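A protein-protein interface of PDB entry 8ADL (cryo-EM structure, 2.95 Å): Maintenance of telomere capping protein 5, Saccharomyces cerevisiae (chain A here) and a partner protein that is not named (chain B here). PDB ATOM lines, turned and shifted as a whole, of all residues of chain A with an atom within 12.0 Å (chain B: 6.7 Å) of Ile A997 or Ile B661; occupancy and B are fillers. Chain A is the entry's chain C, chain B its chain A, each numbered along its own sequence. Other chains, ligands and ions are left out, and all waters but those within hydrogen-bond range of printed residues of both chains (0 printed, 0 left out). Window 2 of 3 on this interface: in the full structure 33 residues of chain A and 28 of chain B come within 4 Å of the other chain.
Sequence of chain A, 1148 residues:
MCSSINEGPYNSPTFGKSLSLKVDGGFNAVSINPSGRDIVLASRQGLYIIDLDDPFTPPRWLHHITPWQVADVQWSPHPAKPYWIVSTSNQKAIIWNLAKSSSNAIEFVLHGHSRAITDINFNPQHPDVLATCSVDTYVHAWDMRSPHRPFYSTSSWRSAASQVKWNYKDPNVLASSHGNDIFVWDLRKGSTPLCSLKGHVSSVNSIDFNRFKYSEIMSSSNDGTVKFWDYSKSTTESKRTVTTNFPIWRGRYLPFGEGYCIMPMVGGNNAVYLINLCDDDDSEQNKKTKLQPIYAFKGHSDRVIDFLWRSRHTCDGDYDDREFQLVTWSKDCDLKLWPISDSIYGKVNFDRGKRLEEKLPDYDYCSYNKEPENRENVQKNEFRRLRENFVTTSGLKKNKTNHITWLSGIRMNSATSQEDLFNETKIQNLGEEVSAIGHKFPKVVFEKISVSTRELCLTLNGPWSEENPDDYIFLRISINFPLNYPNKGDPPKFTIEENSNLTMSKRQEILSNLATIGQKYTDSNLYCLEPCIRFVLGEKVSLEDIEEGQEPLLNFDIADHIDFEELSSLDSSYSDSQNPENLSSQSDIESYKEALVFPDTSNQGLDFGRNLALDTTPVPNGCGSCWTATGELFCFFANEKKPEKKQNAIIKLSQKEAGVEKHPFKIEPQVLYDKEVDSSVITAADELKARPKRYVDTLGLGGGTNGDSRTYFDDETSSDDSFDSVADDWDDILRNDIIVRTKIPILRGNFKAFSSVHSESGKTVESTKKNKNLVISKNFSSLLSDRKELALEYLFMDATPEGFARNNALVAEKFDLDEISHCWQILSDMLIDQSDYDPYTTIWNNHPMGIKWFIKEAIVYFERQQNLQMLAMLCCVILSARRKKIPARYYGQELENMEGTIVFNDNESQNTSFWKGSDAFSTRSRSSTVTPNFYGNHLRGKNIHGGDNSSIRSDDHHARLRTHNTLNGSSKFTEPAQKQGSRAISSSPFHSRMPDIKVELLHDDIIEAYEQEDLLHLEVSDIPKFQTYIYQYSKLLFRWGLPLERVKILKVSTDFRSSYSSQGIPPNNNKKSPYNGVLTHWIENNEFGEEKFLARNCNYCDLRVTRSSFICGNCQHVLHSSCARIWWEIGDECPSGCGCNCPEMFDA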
ATOM      1  N   MET A 994      -9.401  26.319   5.434  1.00  0.00           N
ATOM      2  CA  MET A 994      -9.855  26.674   4.095  1.00  0.00           C
ATOM      3  C   MET A 994      -9.023  27.819   3.517  1.00  0.00           C
ATOM      4  O   MET A 994      -8.680  28.764   4.228  1.00  0.00           O
ATOM      5  CB  MET A 994     -11.341  27.048   4.117  1.00  0.00           C
ATOM      6  CG  MET A 994     -11.724  28.050   5.197  1.00  0.00           C
ATOM      7  SD  MET A 994     -13.507  28.174   5.432  1.00  0.00           S
ATOM      8  CE  MET A 994     -13.780  26.876   6.637  1.00  0.00           C
ATOM      9  N   PRO A 995      -8.685  27.732   2.235  1.00  0.00           N
ATOM     10  CA  PRO A 995      -7.888  28.781   1.595  1.00  0.00           C
ATOM     11  C   PRO A 995      -8.769  29.946   1.153  1.00  0.00           C
ATOM     12  O   PRO A 995      -9.987  29.942   1.324  1.00  0.00           O
ATOM     13  CB  PRO A 995      -7.263  28.056   0.404  1.00  0.00           C
ATOM     14  CG  PRO A 995      -8.276  27.033   0.034  1.00  0.00           C
ATOM     15  CD  PRO A 995      -8.969  26.618   1.310  1.00  0.00           C
ATOM     16  N   ASP A 996      -8.124  30.955   0.573  1.00  0.00           N
ATOM     17  CA  ASP A 996      -8.803  32.133   0.049  1.00  0.00           C
ATOM     18  C   ASP A 996      -8.946  32.010  -1.464  1.00  0.00           C
ATOM     19  O   ASP A 996      -7.953  31.822  -2.174  1.00  0.00           O
ATOM     20  CB  ASP A 996      -8.041  33.406   0.416  1.00  0.00           C
ATOM     21  CG  ASP A 996      -8.018  33.658   1.909  1.00  0.00           C
ATOM     22  OD1 ASP A 996      -8.620  32.860   2.658  1.00  0.00           O
ATOM     23  OD2 ASP A 996      -7.400  34.657   2.337  1.00  0.00           O
ATOM     24  N   ILE A 997     -10.180  32.113  -1.948  1.00  0.00           N
ATOM     25  CA  ILE A 997     -10.507  31.904  -3.352  1.00  0.00           C
ATOM     26  C   ILE A 997     -10.724  33.265  -3.997  1.00  0.00           C
ATOM     27  O   ILE A 997     -11.544  34.061  -3.523  1.00  0.00           O
ATOM     28  CB  ILE A 997     -11.743  31.005  -3.521  1.00  0.00           C
ATOM     29  CG1 ILE A 997     -11.461  29.585  -3.019  1.00  0.00           C
ATOM     30  CG2 ILE A 997     -12.192  30.974  -4.972  1.00  0.00           C
ATOM     31  CD1 ILE A 997     -11.852  29.329  -1.576  1.00  0.00           C
ATOM     32  N   LYS A 998      -9.995  33.537  -5.074  1.00  0.00           N
ATOM     33  CA  LYS A 998     -10.139  34.778  -5.822  1.00  0.00           C
ATOM     34  C   LYS A 998     -10.893  34.515  -7.118  1.00  0.00           C
ATOM     35  O   LYS A 998     -10.519  33.628  -7.893  1.00  0.00           O
ATOM     36  CB  LYS A 998      -8.772  35.395  -6.115  1.00  0.00           C
ATOM     37  CG  LYS A 998      -8.832  36.713  -6.864  1.00  0.00           C
ATOM     38  CD  LYS A 998      -7.482  37.063  -7.466  1.00  0.00           C
ATOM     39  CE  LYS A 998      -7.536  38.393  -8.198  1.00  0.00           C
ATOM     40  NZ  LYS A 998      -6.257  38.694  -8.897  1.00  0.00           N
ATOM     41  N   VAL A 999     -11.952  35.287  -7.348  1.00  0.00           N
ATOM     42  CA  VAL A 999     -12.838  35.122  -8.495  1.00  0.00           C
ATOM     43  C   VAL A 999     -12.737  36.374  -9.353  1.00  0.00           C
ATOM     44  O   VAL A 999     -12.913  37.490  -8.852  1.00  0.00           O
ATOM     45  CB  VAL A 999     -14.293  34.873  -8.055  1.00  0.00           C
ATOM     46  CG1 VAL A 999     -15.209  34.762  -9.266  1.00  0.00           C
ATOM     47  CG2 VAL A 999     -14.381  33.625  -7.189  1.00  0.00           C
ATOM     48  N   GLU A1000     -12.458  36.191 -10.642  1.00  0.00           N
ATOM     49  CA  GLU A1000     -12.296  37.301 -11.581  1.00  0.00           C
ATOM     50  C   GLU A1000     -13.246  37.108 -12.759  1.00  0.00           C
ATOM     51  O   GLU A1000     -12.988  36.285 -13.641  1.00  0.00           O
ATOM     52  CB  GLU A1000     -10.851  37.402 -12.060  1.00  0.00           C
ATOM     53  CG  GLU A1000      -9.939  38.200 -11.145  1.00  0.00           C
ATOM     54  CD  GLU A1000      -8.504  38.219 -11.635  1.00  0.00           C
ATOM     55  OE1 GLU A1000      -8.071  37.220 -12.246  1.00  0.00           O
ATOM     56  OE2 GLU A1000      -7.811  39.234 -11.413  1.00  0.00           O
ATOM     57  N   LEU A1001     -14.340  37.867 -12.770  1.00  0.00           N
ATOM     58  CA  LEU A1001     -15.262  37.846 -13.898  1.00  0.00           C
ATOM     59  C   LEU A1001     -14.616  38.491 -15.119  1.00  0.00           C
ATOM     60  O   LEU A1001     -14.068  39.595 -15.034  1.00  0.00           O
ATOM     61  CB  LEU A1001     -16.555  38.579 -13.545  1.00  0.00           C
ATOM     62  CG  LEU A1001     -17.646  37.815 -12.795  1.00  0.00           C
ATOM     63  CD1 LEU A1001     -18.623  38.784 -12.158  1.00  0.00           C
ATOM     64  CD2 LEU A1001     -18.379  36.881 -13.738  1.00  0.00           C
ATOM     65  N   LEU B 544     -19.625  23.665  -7.726  1.00  0.00           N
ATOM     66  CA  LEU B 544     -18.524  23.508  -8.664  1.00  0.00           C
ATOM     67  C   LEU B 544     -17.269  23.189  -7.869  1.00  0.00           C
ATOM     68  O   LEU B 544     -16.956  23.886  -6.899  1.00  0.00           O
ATOM     69  CB  LEU B 544     -18.328  24.781  -9.496  1.00  0.00           C
ATOM     70  CG  LEU B 544     -17.191  24.812 -10.517  1.00  0.00           C
ATOM     71  CD1 LEU B 544     -17.381  23.744 -11.575  1.00  0.00           C
ATOM     72  CD2 LEU B 544     -17.095  26.187 -11.154  1.00  0.00           C
ATOM     73  N   LEU B 545     -16.555  22.141  -8.271  1.00  0.00           N
ATOM     74  CA  LEU B 545     -15.452  21.611  -7.481  1.00  0.00           C
ATOM     75  C   LEU B 545     -14.104  21.748  -8.167  1.00  0.00           C
ATOM     76  O   LEU B 545     -13.995  21.812  -9.394  1.00  0.00           O
ATOM     77  CB  LEU B 545     -15.681  20.146  -7.087  1.00  0.00           C
ATOM     78  CG  LEU B 545     -16.446  19.904  -5.780  1.00  0.00           C
ATOM     79  CD1 LEU B 545     -17.847  20.359  -5.823  1.00  0.00           C
ATOM     80  CD2 LEU B 545     -16.435  18.422  -5.466  1.00  0.00           C
ATOM     81  N   SER B 546     -13.081  21.791  -7.320  1.00  0.00           N
ATOM     82  CA  SER B 546     -11.683  21.709  -7.698  1.00  0.00           C
ATOM     83  C   SER B 546     -10.973  20.957  -6.583  1.00  0.00           C
ATOM     84  O   SER B 546     -11.597  20.518  -5.613  1.00  0.00           O
ATOM     85  CB  SER B 546     -11.085  23.100  -7.921  1.00  0.00           C
ATOM     86  OG  SER B 546     -11.881  23.852  -8.818  1.00  0.00           O
ATOM     87  N   VAL B 547      -9.661  20.808  -6.716  1.00  0.00           N
ATOM     88  CA  VAL B 547      -8.819  20.410  -5.596  1.00  0.00           C
ATOM     89  C   VAL B 547      -7.670  21.401  -5.484  1.00  0.00           C
ATOM     90  O   VAL B 547      -6.992  21.700  -6.474  1.00  0.00           O
ATOM     91  CB  VAL B 547      -8.312  18.956  -5.725  1.00  0.00           C
ATOM     92  CG1 VAL B 547      -9.440  17.980  -5.437  1.00  0.00           C
ATOM     93  CG2 VAL B 547      -7.762  18.674  -7.109  1.00  0.00           C
ATOM     94  N   ASP B 548      -7.489  21.950  -4.286  1.00  0.00           N
ATOM     95  CA  ASP B 548      -6.393  22.872  -4.008  1.00  0.00           C
ATOM     96  C   ASP B 548      -5.251  22.095  -3.360  1.00  0.00           C
ATOM     97  O   ASP B 548      -4.987  22.179  -2.160  1.00  0.00           O
ATOM     98  CB  ASP B 548      -6.871  24.019  -3.125  1.00  0.00           C
ATOM     99  CG  ASP B 548      -5.836  25.118  -2.990  1.00  0.00           C
ATOM    100  OD1 ASP B 548      -5.072  25.337  -3.952  1.00  0.00           O
ATOM    101  OD2 ASP B 548      -5.789  25.764  -1.921  1.00  0.00           O
ATOM    102  N   CYS B 659      -7.501  20.592  -0.200  1.00  0.00           N
ATOM    103  CA  CYS B 659      -8.788  21.218   0.070  1.00  0.00           C
ATOM    104  C   CYS B 659      -9.634  21.169  -1.193  1.00  0.00           C
ATOM    105  O   CYS B 659      -9.250  21.730  -2.226  1.00  0.00           O
ATOM    106  CB  CYS B 659      -8.607  22.661   0.544  1.00  0.00           C
ATOM    107  SG  CYS B 659      -7.977  22.819   2.230  1.00  0.00           S
ATOM    108  N   ILE B 660     -10.779  20.501  -1.105  1.00  0.00           N
ATOM    109  CA  ILE B 660     -11.763  20.498  -2.183  1.00  0.00           C
ATOM    110  C   ILE B 660     -12.551  21.799  -2.123  1.00  0.00           C
ATOM    111  O   ILE B 660     -13.144  22.133  -1.092  1.00  0.00           O
ATOM    112  CB  ILE B 660     -12.695  19.279  -2.101  1.00  0.00           C
ATOM    113  CG1 ILE B 660     -11.942  17.963  -2.350  1.00  0.00           C
ATOM    114  CG2 ILE B 660     -13.835  19.418  -3.081  1.00  0.00           C
ATOM    115  CD1 ILE B 660     -11.385  17.289  -1.116  1.00  0.00           C
ATOM    116  N   ILE B 661     -12.554  22.535  -3.229  1.00  0.00           N
ATOM    117  CA  ILE B 661     -13.111  23.880  -3.293  1.00  0.00           C
ATOM    118  C   ILE B 661     -14.518  23.767  -3.867  1.00  0.00           C
ATOM    119  O   ILE B 661     -14.703  23.717  -5.085  1.00  0.00           O
ATOM    120  CB  ILE B 661     -12.243  24.811  -4.140  1.00  0.00           C
ATOM    121  CG1 ILE B 661     -10.772  24.691  -3.750  1.00  0.00           C
ATOM    122  CG2 ILE B 661     -12.707  26.244  -3.985  1.00  0.00           C
ATOM    123  CD1 ILE B 661      -9.865  25.549  -4.601  1.00  0.00           C
ATOM    124  N   THR B 662     -15.517  23.743  -2.989  1.00  0.00           N
ATOM    125  CA  THR B 662     -16.912  23.780  -3.403  1.00  0.00           C
ATOM    126  C   THR B 662     -17.360  25.236  -3.410  1.00  0.00           C
ATOM    127  O   THR B 662     -17.322  25.904  -2.371  1.00  0.00           O
ATOM    128  CB  THR B 662     -17.786  22.958  -2.455  1.00  0.00           C
ATOM    129  OG1 THR B 662     -17.726  23.525  -1.142  1.00  0.00           O
ATOM    130  CG2 THR B 662     -17.288  21.527  -2.382  1.00  0.00           C
ATOM    131  N   LEU B 663     -17.785  25.727  -4.571  1.00  0.00           N
ATOM    132  CA  LEU B 663     -18.083  27.140  -4.752  1.00  0.00           C
ATOM    133  C   LEU B 663     -19.537  27.339  -5.145  1.00  0.00           C
ATOM    134  O   LEU B 663     -20.049  26.642  -6.027  1.00  0.00           O
ATOM    135  CB  LEU B 663     -17.179  27.751  -5.825  1.00  0.00           C
ATOM    136  CG  LEU B 663     -15.698  27.863  -5.479  1.00  0.00           C
ATOM    137  CD1 LEU B 663     -14.863  27.906  -6.744  1.00  0.00           C
ATOM    138  CD2 LEU B 663     -15.443  29.091  -4.620  1.00  0.00           C
ATOM    139  N   ILE B 668     -21.607  34.105  -5.465  1.00  0.00           N
ATOM    140  CA  ILE B 668     -20.370  34.864  -5.630  1.00  0.00           C
ATOM    141  C   ILE B 668     -20.498  35.843  -6.790  1.00  0.00           C
ATOM    142  O   ILE B 668     -20.097  37.009  -6.684  1.00  0.00           O
ATOM    143  CB  ILE B 668     -19.180  33.902  -5.814  1.00  0.00           C
ATOM    144  CG1 ILE B 668     -18.890  33.163  -4.506  1.00  0.00           C
ATOM    145  CG2 ILE B 668     -17.937  34.638  -6.289  1.00  0.00           C
ATOM    146  CD1 ILE B 668     -17.920  32.012  -4.656  1.00  0.00           C
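Of the 11 printed residues of chain B, 4 touch a printed residue of chain A. Printed residues of chain B that touch a printed residue of chain A: Asp B548, Ile B661, Leu B663 and Ile B668. Printed residues of chain A that touch a printed residue of chain B: Pro A995, Ile A997 and Val A999. Among the printed residues, no Asp or Glu carboxylate lies within 4 Å of a Lys or Arg side-chain nitrogen of the other chain.
Among the printed residues, pairs that only touch across the chains: Pro A995 with Asp B548 (3.4 Å), Ile A997 with Ile B661 (3.7 Å), Ile A997 with Leu B663 (3.8 Å) and Val A999 with Ile B668 (3.8 Å).
Met A994 touches none of the printed residues of chain B. Printed residues of chain B within 4 Å of Pro A995: Asp B548. Ile A997 touches just these residues of chain B: Ile B661 and Leu B663. Printed residues of chain B within 4 Å of Val A999: Ile B668 (3.8 Å). Glu A1000 touches none of the printed residues of chain B. No residue of chain A comes within 4 Å of Leu B544. Leu B545 touches none of the printed residues of chain A. Ser B546 touches none of the printed residues of chain A. No residue of chain A comes within 4 Å of Val B547. Of the printed residues of chain A, Asp B548 touches Pro A995 (3.4 Å). Cys B659 touches none of the printed residues of chain A. Ile B661 touches just one residue of chain A: Ile A997 (3.7 Å). Thr B662 touches none of the printed residues of chain A. Printed residues of chain A within 4 Å of Ile B668: Val A999.
N of Leu B663 sits at hydrogen-bond distance from O of Leu B544, 3.1 Å away. O of Cys B659 is in hydrogen-bond range of N of Asp B548, 2.7 Å away. The backbone NH of Ile B661 lies within hydrogen-bond range of the backbone carbonyl oxygen of Ser B546 (3.3 Å).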
